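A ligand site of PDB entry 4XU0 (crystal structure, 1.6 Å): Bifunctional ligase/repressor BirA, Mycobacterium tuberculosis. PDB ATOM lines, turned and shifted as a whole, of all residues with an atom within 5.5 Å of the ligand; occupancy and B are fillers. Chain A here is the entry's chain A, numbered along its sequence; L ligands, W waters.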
ATOM      1  N   GLY A  41      12.511 -26.252  15.878  1.00  0.00           N
ATOM      2  CA  GLY A  41      12.969 -25.439  16.992  1.00  0.00           C
ATOM      3  C   GLY A  41      14.344 -24.869  16.729  1.00  0.00           C
ATOM      4  O   GLY A  41      14.558 -23.665  16.812  1.00  0.00           O
ATOM      5  N   SER A  42      15.289 -25.747  16.410  1.00  0.00           N
ATOM      6  CA  SER A  42      16.652 -25.335  16.107  1.00  0.00           C
ATOM      7  C   SER A  42      17.334 -26.400  15.254  1.00  0.00           C
ATOM      8  O   SER A  42      17.416 -27.554  15.652  1.00  0.00           O
ATOM      9  CB  SER A  42      17.452 -25.109  17.390  1.00  0.00           C
ATOM     10  OG  SER A  42      18.844 -25.107  17.135  1.00  0.00           O
ATOM     11  N   THR A  43      17.815 -26.001  14.075  1.00  0.00           N
ATOM     12  CA  THR A  43      18.480 -26.938  13.182  1.00  0.00           C
ATOM     13  C   THR A  43      19.750 -27.507  13.807  1.00  0.00           C
ATOM     14  O   THR A  43      20.080 -28.669  13.593  1.00  0.00           O
ATOM     15  CB  THR A  43      18.843 -26.288  11.830  1.00  0.00           C
ATOM     16  OG1 THR A  43      19.685 -25.162  12.058  1.00  0.00           O
ATOM     17  CG2 THR A  43      17.582 -25.855  11.099  1.00  0.00           C
ATOM     18  N   ASN A  44      20.448 -26.681  14.578  1.00  0.00           N
ATOM     19  CA  ASN A  44      21.625 -27.157  15.299  1.00  0.00           C
ATOM     20  C   ASN A  44      21.254 -28.252  16.296  1.00  0.00           C
ATOM     21  O   ASN A  44      21.895 -29.293  16.336  1.00  0.00           O
ATOM     22  CB  ASN A  44      22.331 -26.009  16.022  1.00  0.00           C
ATOM     23  CG  ASN A  44      23.514 -25.468  15.245  1.00  0.00           C
ATOM     24  OD1 ASN A  44      23.514 -25.500  14.021  1.00  0.00           O
ATOM     25  ND2 ASN A  44      24.512 -24.982  15.958  1.00  0.00           N
ATOM     26  N   ALA A  45      20.213 -28.006  17.084  1.00  0.00           N
ATOM     27  CA  ALA A  45      19.730 -29.000  18.035  1.00  0.00           C
ATOM     28  C   ALA A  45      19.319 -30.289  17.327  1.00  0.00           C
ATOM     29  O   ALA A  45      19.588 -31.386  17.833  1.00  0.00           O
ATOM     30  CB  ALA A  45      18.559 -28.442  18.824  1.00  0.00           C
ATOM     31  N   GLN A  67      12.358 -21.127  11.917  1.00  0.00           N
ATOM     32  CA  GLN A  67      12.984 -21.638  13.124  1.00  0.00           C
ATOM     33  C   GLN A  67      12.433 -20.904  14.346  1.00  0.00           C
ATOM     34  O   GLN A  67      12.612 -19.692  14.482  1.00  0.00           O
ATOM     35  CB  GLN A  67      14.505 -21.478  13.044  1.00  0.00           C
ATOM     36  CG  GLN A  67      15.276 -22.221  14.113  1.00  0.00           C
ATOM     37  CD  GLN A  67      16.769 -22.133  13.924  1.00  0.00           C
ATOM     38  OE1 GLN A  67      17.429 -23.132  13.638  1.00  0.00           O
ATOM     39  NE2 GLN A  67      17.317 -20.934  14.074  1.00  0.00           N
ATOM     40  N   ALA A  69      12.779 -21.664  17.830  1.00  0.00           N
ATOM     41  CA  ALA A  69      13.548 -21.607  19.068  1.00  0.00           C
ATOM     42  C   ALA A  69      15.043 -21.535  18.773  1.00  0.00           C
ATOM     43  O   ALA A  69      15.830 -22.302  19.329  1.00  0.00           O
ATOM     44  CB  ALA A  69      13.233 -22.805  19.955  1.00  0.00           C
ATOM     45  N   GLY A  70      15.412 -20.617  17.892  1.00  0.00           N
ATOM     46  CA  GLY A  70      16.792 -20.488  17.449  1.00  0.00           C
ATOM     47  C   GLY A  70      17.776 -20.210  18.577  1.00  0.00           C
ATOM     48  O   GLY A  70      17.435 -19.542  19.559  1.00  0.00           O
ATOM     49  N   ARG A  71      18.989 -20.734  18.437  1.00  0.00           N
ATOM     50  CA  ARG A  71      20.000 -20.566  19.459  1.00  0.00           C
ATOM     51  C   ARG A  71      21.173 -19.721  18.965  1.00  0.00           C
ATOM     52  O   ARG A  71      21.674 -19.911  17.863  1.00  0.00           O
ATOM     53  CB  ARG A  71      20.515 -21.924  19.934  1.00  0.00           C
ATOM     54  CG  ARG A  71      19.442 -22.794  20.564  1.00  0.00           C
ATOM     55  CD  ARG A  71      20.050 -24.092  21.095  1.00  0.00           C
ATOM     56  NE  ARG A  71      20.641 -24.887  20.029  1.00  0.00           N
ATOM     57  CZ  ARG A  71      21.347 -25.999  20.234  1.00  0.00           C
ATOM     58  NH1 ARG A  71      21.525 -26.442  21.476  1.00  0.00           N
ATOM     59  NH2 ARG A  71      21.847 -26.664  19.196  1.00  0.00           N
ATOM     60  N   GLY A  72      21.581 -18.764  19.799  1.00  0.00           N
ATOM     61  CA  GLY A  72      22.776 -17.981  19.546  1.00  0.00           C
ATOM     62  C   GLY A  72      23.909 -18.473  20.420  1.00  0.00           C
ATOM     63  O   GLY A  72      23.762 -19.464  21.145  1.00  0.00           O
ATOM     64  N   ARG A  73      25.043 -17.798  20.367  1.00  0.00           N
ATOM     65  CA  ARG A  73      26.178 -18.151  21.205  1.00  0.00           C
ATOM     66  C   ARG A  73      25.908 -17.790  22.662  1.00  0.00           C
ATOM     67  O   ARG A  73      25.120 -16.879  22.946  1.00  0.00           O
ATOM     68  CB  ARG A  73      27.454 -17.462  20.713  1.00  0.00           C
ATOM     69  CG  ARG A  73      27.873 -17.878  19.317  1.00  0.00           C
ATOM     70  CD  ARG A  73      29.271 -17.400  18.960  1.00  0.00           C
ATOM     71  NE  ARG A  73      29.336 -15.953  18.751  1.00  0.00           N
ATOM     72  CZ  ARG A  73      29.069 -15.350  17.600  1.00  0.00           C
ATOM     73  NH1 ARG A  73      28.699 -16.058  16.544  1.00  0.00           N
ATOM     74  NH2 ARG A  73      29.168 -14.032  17.507  1.00  0.00           N
ATOM     75  N   HIS A  74      26.538 -18.514  23.566  1.00  0.00           N
ATOM     76  CA  HIS A  74      26.488 -18.231  24.998  1.00  0.00           C
ATOM     77  C   HIS A  74      25.065 -18.188  25.555  1.00  0.00           C
ATOM     78  O   HIS A  74      24.749 -17.330  26.389  1.00  0.00           O
ATOM     79  CB  HIS A  74      27.206 -16.911  25.294  1.00  0.00           C
ATOM     80  CG  HIS A  74      28.541 -16.795  24.638  1.00  0.00           C
ATOM     81  ND1 HIS A  74      29.615 -17.586  24.988  1.00  0.00           N
ATOM     82  CD2 HIS A  74      28.983 -15.992  23.648  1.00  0.00           C
ATOM     83  CE1 HIS A  74      30.658 -17.269  24.253  1.00  0.00           C
ATOM     84  NE2 HIS A  74      30.298 -16.305  23.420  1.00  0.00           N
ATOM     85  N   ARG A  76      22.338 -17.332  24.156  1.00  0.00           N
ATOM     86  CA  ARG A  76      21.468 -16.305  23.590  1.00  0.00           C
ATOM     87  C   ARG A  76      20.529 -16.912  22.564  1.00  0.00           C
ATOM     88  O   ARG A  76      20.598 -18.101  22.262  1.00  0.00           O
ATOM     89  CB  ARG A  76      22.297 -15.183  22.946  1.00  0.00           C
ATOM     90  CG  ARG A  76      23.006 -14.305  23.967  1.00  0.00           C
ATOM     91  CD  ARG A  76      23.625 -13.063  23.316  1.00  0.00           C
ATOM     92  NE  ARG A  76      24.834 -13.379  22.560  1.00  0.00           N
ATOM     93  CZ  ARG A  76      26.063 -13.253  23.051  1.00  0.00           C
ATOM     94  NH1 ARG A  76      26.252 -12.816  24.283  1.00  0.00           N
ATOM     95  NH2 ARG A  76      27.111 -13.565  22.287  1.00  0.00           N
ATOM     96  N   GLY A  77      19.633 -16.088  22.027  1.00  0.00           N
ATOM     97  CA  GLY A  77      18.657 -16.565  21.061  1.00  0.00           C
ATOM     98  C   GLY A  77      18.927 -16.097  19.647  1.00  0.00           C
ATOM     99  O   GLY A  77      19.723 -15.194  19.412  1.00  0.00           O
ATOM    100  N   TRP A  78      18.259 -16.743  18.695  1.00  0.00           N
ATOM    101  CA  TRP A  78      18.286 -16.312  17.304  1.00  0.00           C
ATOM    102  C   TRP A  78      16.859 -16.239  16.787  1.00  0.00           C
ATOM    103  O   TRP A  78      16.137 -17.236  16.806  1.00  0.00           O
ATOM    104  CB  TRP A  78      19.116 -17.256  16.433  1.00  0.00           C
ATOM    105  CG  TRP A  78      19.337 -16.754  15.042  1.00  0.00           C
ATOM    106  CD1 TRP A  78      18.712 -17.170  13.900  1.00  0.00           C
ATOM    107  CD2 TRP A  78      20.249 -15.717  14.644  1.00  0.00           C
ATOM    108  NE1 TRP A  78      19.179 -16.473  12.821  1.00  0.00           N
ATOM    109  CE2 TRP A  78      20.121 -15.568  13.245  1.00  0.00           C
ATOM    110  CE3 TRP A  78      21.154 -14.910  15.331  1.00  0.00           C
ATOM    111  CZ2 TRP A  78      20.873 -14.639  12.526  1.00  0.00           C
ATOM    112  CZ3 TRP A  78      21.898 -13.985  14.605  1.00  0.00           C
ATOM    113  CH2 TRP A  78      21.756 -13.862  13.219  1.00  0.00           C
ATOM    114  N   ALA A  79      16.448 -15.058  16.341  1.00  0.00           N
ATOM    115  CA  ALA A  79      15.080 -14.841  15.895  1.00  0.00           C
ATOM    116  C   ALA A  79      14.956 -14.967  14.381  1.00  0.00           C
ATOM    117  O   ALA A  79      15.903 -14.700  13.637  1.00  0.00           O
ATOM    118  CB  ALA A  79      14.586 -13.481  16.349  1.00  0.00           C
ATOM    119  N   ALA A  80      13.774 -15.385  13.925  1.00  0.00           N
ATOM    120  CA  ALA A  80      13.516 -15.544  12.500  1.00  0.00           C
ATOM    121  C   ALA A  80      12.025 -15.525  12.208  1.00  0.00           C
ATOM    122  O   ALA A  80      11.203 -15.854  13.061  1.00  0.00           O
ATOM    123  CB  ALA A  80      14.136 -16.841  12.001  1.00  0.00           C
ATOM    124  N   GLN A  85      15.029 -15.960   5.968  1.00  0.00           N
ATOM    125  CA  GLN A  85      16.444 -16.253   6.126  1.00  0.00           C
ATOM    126  C   GLN A  85      16.835 -17.569   5.467  1.00  0.00           C
ATOM    127  O   GLN A  85      15.985 -18.384   5.120  1.00  0.00           O
ATOM    128  CB  GLN A  85      16.826 -16.355   7.610  1.00  0.00           C
ATOM    129  CG  GLN A  85      16.616 -15.123   8.450  1.00  0.00           C
ATOM    130  CD  GLN A  85      17.045 -15.356   9.894  1.00  0.00           C
ATOM    131  OE1 GLN A  85      17.942 -16.155  10.163  1.00  0.00           O
ATOM    132  NE2 GLN A  85      16.397 -14.669  10.821  1.00  0.00           N
ATOM    133  N   ILE A  87      18.388 -20.625   6.883  1.00  0.00           N
ATOM    134  CA  ILE A  87      18.619 -21.193   8.201  1.00  0.00           C
ATOM    135  C   ILE A  87      19.083 -22.633   8.042  1.00  0.00           C
ATOM    136  O   ILE A  87      18.283 -23.514   7.731  1.00  0.00           O
ATOM    137  CB  ILE A  87      17.330 -21.166   9.056  1.00  0.00           C
ATOM    138  CG1 ILE A  87      16.835 -19.730   9.237  1.00  0.00           C
ATOM    139  CG2 ILE A  87      17.553 -21.827  10.412  1.00  0.00           C
ATOM    140  CD1 ILE A  87      15.479 -19.643   9.918  1.00  0.00           C
ATOM    141  N   LEU A  88      20.383 -22.882   8.247  1.00  0.00           N
ATOM    142  CA  LEU A  88      20.884 -24.233   8.050  1.00  0.00           C
ATOM    143  C   LEU A  88      21.959 -24.666   9.042  1.00  0.00           C
ATOM    144  O   LEU A  88      22.627 -23.841   9.673  1.00  0.00           O
ATOM    145  CB  LEU A  88      21.411 -24.401   6.624  1.00  0.00           C
ATOM    146  CG  LEU A  88      22.559 -23.541   6.071  1.00  0.00           C
ATOM    147  CD1 LEU A  88      23.922 -24.069   6.493  1.00  0.00           C
ATOM    148  CD2 LEU A  88      22.467 -23.506   4.556  1.00  0.00           C
ATOM    149  N   SER A  89      22.084 -25.976   9.161  1.00  0.00           N
ATOM    150  CA  SER A  89      23.141 -26.605   9.947  1.00  0.00           C
ATOM    151  C   SER A  89      23.788 -27.702   9.118  1.00  0.00           C
ATOM    152  O   SER A  89      23.108 -28.372   8.333  1.00  0.00           O
ATOM    153  CB  SER A  89      22.590 -27.169  11.251  1.00  0.00           C
ATOM    154  OG  SER A  89      22.074 -26.145  12.076  1.00  0.00           O
ATOM    155  N   ASN A 134      32.336 -14.880  14.923  1.00  0.00           N
ATOM    156  CA  ASN A 134      31.479 -15.295  13.825  1.00  0.00           C
ATOM    157  C   ASN A 134      30.293 -14.373  13.573  1.00  0.00           C
ATOM    158  O   ASN A 134      29.135 -14.772  13.731  1.00  0.00           O
ATOM    159  CB  ASN A 134      30.973 -16.708  14.077  1.00  0.00           C
ATOM    160  CG  ASN A 134      31.728 -17.735  13.266  1.00  0.00           C
ATOM    161  OD1 ASN A 134      31.708 -18.917  13.571  1.00  0.00           O
ATOM    162  ND2 ASN A 134      32.406 -17.279  12.216  1.00  0.00           N
ATOM    163  N   ASP A 135      30.597 -13.149  13.163  1.00  0.00           N
ATOM    164  CA  ASP A 135      29.582 -12.222  12.714  1.00  0.00           C
ATOM    165  C   ASP A 135      29.906 -11.755  11.302  1.00  0.00           C
ATOM    166  O   ASP A 135      30.994 -11.247  11.046  1.00  0.00           O
ATOM    167  CB  ASP A 135      29.489 -11.017  13.656  1.00  0.00           C
ATOM    168  CG  ASP A 135      28.680 -11.315  14.908  1.00  0.00           C
ATOM    169  OD1 ASP A 135      28.483 -12.503  15.243  1.00  0.00           O
ATOM    170  OD2 ASP A 135      28.243 -10.348  15.574  1.00  0.00           O
ATOM    171  N   LYS A 142      24.402  -6.605  11.418  1.00  0.00           N
ATOM    172  CA  LYS A 142      24.660  -8.037  11.458  1.00  0.00           C
ATOM    173  C   LYS A 142      23.845  -8.760  10.392  1.00  0.00           C
ATOM    174  O   LYS A 142      22.623  -8.904  10.520  1.00  0.00           O
ATOM    175  CB  LYS A 142      24.362  -8.602  12.840  1.00  0.00           C
ATOM    176  CG  LYS A 142      24.682 -10.085  12.975  1.00  0.00           C
ATOM    177  CD  LYS A 142      24.813 -10.498  14.416  1.00  0.00           C
ATOM    178  CE  LYS A 142      25.202 -11.955  14.541  1.00  0.00           C
ATOM    179  NZ  LYS A 142      25.442 -12.332  15.949  1.00  0.00           N
ATOM    180  N   ALA A 144      24.635 -11.977   9.229  1.00  0.00           N
ATOM    181  CA  ALA A 144      24.582 -13.406   9.527  1.00  0.00           C
ATOM    182  C   ALA A 144      25.259 -13.743  10.849  1.00  0.00           C
ATOM    183  O   ALA A 144      26.219 -13.084  11.256  1.00  0.00           O
ATOM    184  CB  ALA A 144      25.212 -14.214   8.393  1.00  0.00           C
ATOM    185  N   GLY A 145      24.768 -14.774  11.509  1.00  0.00           N
ATOM    186  CA  GLY A 145      25.368 -15.271  12.739  1.00  0.00           C
ATOM    187  C   GLY A 145      25.697 -16.730  12.583  1.00  0.00           C
ATOM    188  O   GLY A 145      24.953 -17.484  11.959  1.00  0.00           O
ATOM    189  N   ILE A 146      26.834 -17.144  13.146  1.00  0.00           N
ATOM    190  CA  ILE A 146      27.287 -18.524  13.051  1.00  0.00           C
ATOM    191  C   ILE A 146      27.437 -19.154  14.427  1.00  0.00           C
ATOM    192  O   ILE A 146      27.970 -18.531  15.353  1.00  0.00           O
ATOM    193  CB  ILE A 146      28.629 -18.637  12.302  1.00  0.00           C
ATOM    194  CG1 ILE A 146      28.619 -17.760  11.048  1.00  0.00           C
ATOM    195  CG2 ILE A 146      28.944 -20.085  11.967  1.00  0.00           C
ATOM    196  CD1 ILE A 146      27.604 -18.166  10.014  1.00  0.00           C
ATOM    197  N   LEU A 147      26.992 -20.400  14.563  1.00  0.00           N
ATOM    198  CA  LEU A 147      27.071 -21.116  15.823  1.00  0.00           C
ATOM    199  C   LEU A 147      27.636 -22.516  15.641  1.00  0.00           C
ATOM    200  O   LEU A 147      27.065 -23.330  14.911  1.00  0.00           O
ATOM    201  CB  LEU A 147      25.698 -21.201  16.493  1.00  0.00           C
ATOM    202  CG  LEU A 147      25.641 -21.990  17.799  1.00  0.00           C
ATOM    203  CD1 LEU A 147      26.478 -21.319  18.880  1.00  0.00           C
ATOM    204  CD2 LEU A 147      24.196 -22.146  18.266  1.00  0.00           C
ATOM    205  N   GLY A 158      26.152 -24.005  12.473  1.00  0.00           N
ATOM    206  CA  GLY A 158      24.859 -23.398  12.189  1.00  0.00           C
ATOM    207  C   GLY A 158      24.997 -22.016  11.593  1.00  0.00           C
ATOM    208  O   GLY A 158      25.770 -21.197  12.076  1.00  0.00           O
ATOM    209  N   VAL A 159      24.246 -21.762  10.523  1.00  0.00           N
ATOM    210  CA  VAL A 159      24.236 -20.461   9.863  1.00  0.00           C
ATOM    211  C   VAL A 159      22.845 -19.847   9.815  1.00  0.00           C
ATOM    212  O   VAL A 159      21.885 -20.485   9.382  1.00  0.00           O
ATOM    213  CB  VAL A 159      24.775 -20.552   8.418  1.00  0.00           C
ATOM    214  CG1 VAL A 159      24.701 -19.188   7.740  1.00  0.00           C
ATOM    215  CG2 VAL A 159      26.205 -21.069   8.409  1.00  0.00           C
ATOM    216  N   GLY A 160      22.739 -18.611  10.280  1.00  0.00           N
ATOM    217  CA  GLY A 160      21.523 -17.838  10.149  1.00  0.00           C
ATOM    218  C   GLY A 160      21.833 -16.613   9.319  1.00  0.00           C
ATOM    219  O   GLY A 160      22.478 -15.679   9.798  1.00  0.00           O
ATOM    220  N   ASN A 162      20.419 -13.423   7.127  1.00  0.00           N
ATOM    221  CA  ASN A 162      19.263 -12.570   6.842  1.00  0.00           C
ATOM    222  C   ASN A 162      19.172 -12.229   5.358  1.00  0.00           C
ATOM    223  O   ASN A 162      19.989 -11.461   4.846  1.00  0.00           O
ATOM    224  CB  ASN A 162      19.326 -11.282   7.662  1.00  0.00           C
ATOM    225  CG  ASN A 162      19.299 -11.532   9.157  1.00  0.00           C
ATOM    226  OD1 ASN A 162      20.071 -10.922   9.897  1.00  0.00           O
ATOM    227  ND2 ASN A 162      18.407 -12.396   9.610  1.00  0.00           N
ATOM    228  N   GLN A 165      14.974 -10.664   5.815  1.00  0.00           N
ATOM    229  CA  GLN A 165      14.579 -10.454   7.199  1.00  0.00           C
ATOM    230  C   GLN A 165      14.662  -8.983   7.577  1.00  0.00           C
ATOM    231  O   GLN A 165      15.728  -8.373   7.505  1.00  0.00           O
ATOM    232  CB  GLN A 165      15.453 -11.295   8.134  1.00  0.00           C
ATOM    233  CG  GLN A 165      14.963 -11.345   9.573  1.00  0.00           C
ATOM    234  CD  GLN A 165      13.777 -12.260   9.750  1.00  0.00           C
ATOM    235  OE1 GLN A 165      13.938 -13.474   9.878  1.00  0.00           O
ATOM    236  NE2 GLN A 165      12.581 -11.693   9.754  1.00  0.00           N
ATOM    237  N   VAL A 170      13.733  -8.820  14.196  1.00  0.00           N
ATOM    238  CA  VAL A 170      14.728  -9.656  14.863  1.00  0.00           C
ATOM    239  C   VAL A 170      15.683  -8.924  15.812  1.00  0.00           C
ATOM    240  O   VAL A 170      15.885  -9.365  16.947  1.00  0.00           O
ATOM    241  CB  VAL A 170      15.582 -10.426  13.819  1.00  0.00           C
ATOM    242  CG1 VAL A 170      14.782 -11.592  13.260  1.00  0.00           C
ATOM    243  CG2 VAL A 170      16.031  -9.503  12.702  1.00  0.00           C
ATOM    244  N   ASP A 171      16.270  -7.818  15.357  1.00  0.00           N
ATOM    245  CA  ASP A 171      17.254  -7.082  16.161  1.00  0.00           C
ATOM    246  C   ASP A 171      17.544  -5.717  15.559  1.00  0.00           C
ATOM    247  O   ASP A 171      17.649  -5.579  14.342  1.00  0.00           O
ATOM    248  CB  ASP A 171      18.551  -7.897  16.283  1.00  0.00           C
ATOM    249  CG  ASP A 171      19.507  -7.313  17.301  1.00  0.00           C
ATOM    250  OD1 ASP A 171      19.355  -7.619  18.506  1.00  0.00           O
ATOM    251  OD2 ASP A 171      20.419  -6.554  16.907  1.00  0.00           O
ATOM    252  N   ALA A 174      20.549  -5.521  13.324  1.00  0.00           N
ATOM    253  CA  ALA A 174      20.522  -6.468  12.226  1.00  0.00           C
ATOM    254  C   ALA A 174      20.394  -5.781  10.876  1.00  0.00           C
ATOM    255  O   ALA A 174      19.971  -4.623  10.787  1.00  0.00           O
ATOM    256  CB  ALA A 174      19.391  -7.460  12.407  1.00  0.00           C
ATOM    257  N   THR A 175      20.762  -6.494   9.822  1.00  0.00           N
ATOM    258  CA  THR A 175      20.524  -6.055   8.460  1.00  0.00           C
ATOM    259  C   THR A 175      20.245  -7.279   7.603  1.00  0.00           C
ATOM    260  O   THR A 175      20.368  -8.407   8.084  1.00  0.00           O
ATOM    261  CB  THR A 175      21.716  -5.259   7.887  1.00  0.00           C
ATOM    262  OG1 THR A 175      21.319  -4.631   6.651  1.00  0.00           O
ATOM    263  CG2 THR A 175      22.905  -6.176   7.625  1.00  0.00           C
ATOM    264  N   ASP A 265      32.261 -11.165  23.085  1.00  0.00           N
ATOM    265  CA  ASP A 265      31.520 -10.312  22.168  1.00  0.00           C
ATOM    266  C   ASP A 265      32.328  -9.059  21.852  1.00  0.00           C
ATOM    267  O   ASP A 265      32.725  -8.334  22.759  1.00  0.00           O
ATOM    268  CB  ASP A 265      30.154  -9.946  22.746  1.00  0.00           C
ATOM    269  CG  ASP A 265      29.319 -11.159  23.074  1.00  0.00           C
ATOM    270  OD1 ASP A 265      29.328 -12.119  22.289  1.00  0.00           O
ATOM    271  OD2 ASP A 265      28.660 -11.154  24.141  1.00  0.00           O
HETATM  272  C1  LIG L   1      20.619 -10.450  13.464  1.00  0.00           C
HETATM  273  C2  LIG L   1      19.042 -12.135  14.875  1.00  0.00           C
HETATM  274  C3  LIG L   1      19.974 -11.347  15.523  1.00  0.00           C
HETATM  275  N1  LIG L   1      20.743 -10.504  14.792  1.00  0.00           N
HETATM  276  C4  LIG L   1      18.954 -12.522  17.013  1.00  0.00           C
HETATM  277  N2  LIG L   1      19.728 -11.210  12.819  1.00  0.00           N
HETATM  278  C5  LIG L   1      18.925 -12.060  13.497  1.00  0.00           C
HETATM  279  C6  LIG L   1      22.014 -21.571  14.265  1.00  0.00           C
HETATM  280  N3  LIG L   1      21.331 -21.566  15.550  1.00  0.00           N
HETATM  281  C7  LIG L   1      20.371 -22.484  15.597  1.00  0.00           C
HETATM  282  O1  LIG L   1      19.535 -22.582  16.486  1.00  0.00           O
HETATM  283  N4  LIG L   1      20.421 -23.245  14.515  1.00  0.00           N
HETATM  284  C8  LIG L   1      21.270 -22.669  13.500  1.00  0.00           C
HETATM  285  C9  LIG L   1      20.393 -22.125  12.390  1.00  0.00           C
HETATM  286  S1  LIG L   1      20.456 -20.382  12.584  1.00  0.00           S
HETATM  287  C10 LIG L   1      21.920 -20.232  13.542  1.00  0.00           C
HETATM  288  C11 LIG L   1      21.918 -19.066  14.523  1.00  0.00           C
HETATM  289  C12 LIG L   1      23.349 -18.821  14.999  1.00  0.00           C
HETATM  290  C13 LIG L   1      23.475 -17.477  15.705  1.00  0.00           C
HETATM  291  C14 LIG L   1      24.866 -17.305  16.323  1.00  0.00           C
HETATM  292  C15 LIG L   1      24.994 -15.910  16.876  1.00  0.00           C
HETATM  293  O2  LIG L   1      25.066 -14.951  16.125  1.00  0.00           O
HETATM  294  N5  LIG L   1      25.002 -15.804  18.198  1.00  0.00           N
HETATM  295  S2  LIG L   1      25.335 -14.408  18.913  1.00  0.00           S
HETATM  296  O3  LIG L   1      26.577 -13.890  18.412  1.00  0.00           O
HETATM  297  O4  LIG L   1      25.461 -14.613  20.325  1.00  0.00           O
HETATM  298  O5  LIG L   1      24.249 -13.372  18.637  1.00  0.00           O
HETATM  299  C16 LIG L   1      22.881 -13.577  18.991  1.00  0.00           C
HETATM  300  C17 LIG L   1      22.276 -12.176  19.124  1.00  0.00           C
HETATM  301  O6  LIG L   1      22.022 -11.608  17.832  1.00  0.00           O
HETATM  302  C18 LIG L   1      20.951 -12.125  19.865  1.00  0.00           C
HETATM  303  O7  LIG L   1      21.177 -11.983  21.272  1.00  0.00           O
HETATM  304  C19 LIG L   1      20.341 -10.864  19.292  1.00  0.00           C
HETATM  305  O8  LIG L   1      21.015  -9.749  19.891  1.00  0.00           O
HETATM  306  C20 LIG L   1      18.854 -10.717  19.586  1.00  0.00           C
HETATM  307  C21 LIG L   1      20.774 -10.897  17.828  1.00  0.00           C
HETATM  308  N6  LIG L   1      19.897 -11.585  16.833  1.00  0.00           N
HETATM  309  N7  LIG L   1      18.412 -12.865  15.822  1.00  0.00           N
HETATM  310  N8  LIG L   1      18.022 -12.819  12.818  1.00  0.00           N
HETATM  311  O   HOH W   1      19.218 -13.330  22.611  1.00  0.00           O
HETATM  312  O   HOH W   2      22.237  -8.065  15.585  1.00  0.00           O
HETATM  313  O   HOH W   3      16.890 -13.477  19.558  1.00  0.00           O
HETATM  314  O   HOH W   4      25.239 -10.136  17.791  1.00  0.00           O
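Water W1 lies within hydrogen-bond range of an oxygen (O7) of the ligand (2.7 Å) and the backbone NH of Gly 77 (2.8 Å).
Water W2 bridges OD2 of Asp 171 (2.7 Å) and N1 of the ligand (3.0 Å).
Water W4 lies within hydrogen-bond range of NZ of Lys 142 (2.9 Å) and O5 of the ligand (3.5 Å).
The guanidinium group of Arg 73 is in hydrogen-bond range of the backbone carbonyl oxygen of Asn 134 (3.1 Å).
The side-chain amide nitrogen (NE2) of Gln 85 is in hydrogen-bond range of the backbone carbonyl oxygen (O) of Ala 79 (2.9 Å).
OG of Ser 89 is in hydrogen-bond range of OG1 of Thr 43 (2.6 Å).
The backbone carbonyl oxygen of Gly 145 lies within hydrogen-bond range of the backbone NH of Gly 160 (3.0 Å).
The backbone NH of Ile 146 is in hydrogen-bond range of the backbone carbonyl oxygen of Asn 134.
The backbone NH (N) of Val 159 sits at hydrogen-bond distance from the backbone carbonyl oxygen (O) of Leu 88, at 2.8 Å.
The backbone NH (N) of Gly 70 is in hydrogen-bond range of the backbone carbonyl oxygen (O) of Gly 41 (3.3 Å).
The backbone carbonyl oxygen of Leu 147 lies within hydrogen-bond range of the backbone NH of Gly 158, 2.7 Å away.
O4 of the ligand sits at hydrogen-bond distance from NE of Arg 76, 2.6 Å away.
The side-chain amino group of Lys 142 sits at hydrogen-bond distance from an oxygen (O2) of the ligand.
An oxygen (O1) of the ligand lies within hydrogen-bond range of the side-chain hydroxyl (OG) of Ser 42 (2.7 Å).
N of Arg 71 lies within hydrogen-bond range of O1 of the ligand (2.7 Å).
O of Arg 71 is in hydrogen-bond range of N3 of the ligand, 2.9 Å away.
N of Arg 73 sits at hydrogen-bond distance from N5 of the ligand (2.9 Å).
An oxygen (O3) of the ligand is in hydrogen-bond range of the guanidinium group of Arg 73, 2.7 Å away.
The backbone NH (N) of Ala 79 is in hydrogen-bond range of a nitrogen (N7) of the ligand.
The backbone carbonyl oxygen of Ala 79 sits at hydrogen-bond distance from a nitrogen (N8) of the ligand (2.9 Å).
OD1 of Asn 162 sits close to N2 of the ligand, at 3.0 Å.
OD1 of Asp 171 is in hydrogen-bond range of O8 of the ligand (3.0 Å).
A nitrogen (N4) of the ligand sits at hydrogen-bond distance from the side-chain amide oxygen (OE1) of Gln 67 (3.1 Å).
The side-chain hydroxyl of Thr 43 lies close to a nitrogen (N4) of the ligand (3.2 Å).
NE2 of Gln 85 lies close to N8 of the ligand (3.2 Å).
S1 of the ligand lies close to N of Gly 160, 3.7 Å away.
N4 of the ligand lies close to N of Asn 44.
A sulfur (S1) of the ligand sits close to the backbone carbonyl oxygen (O) of Val 159 (3.5 Å).
Residues that only touch the ligand: Gly 70, Gly 72, Gly 77, Trp 78, Ile 87, Leu 88, Ser 89, Asp 135, Gly 145, Ile 146, Leu 147, Gly 158, Val 170 and Ala 174.
Hydrophobic or aromatic side chains that line the ligand: Trp 78, Ala 79, Ile 87, Leu 147, Val 170 and Ala 174.
Of the 38 residues printed, 28 come within 4 Å of the ligand.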
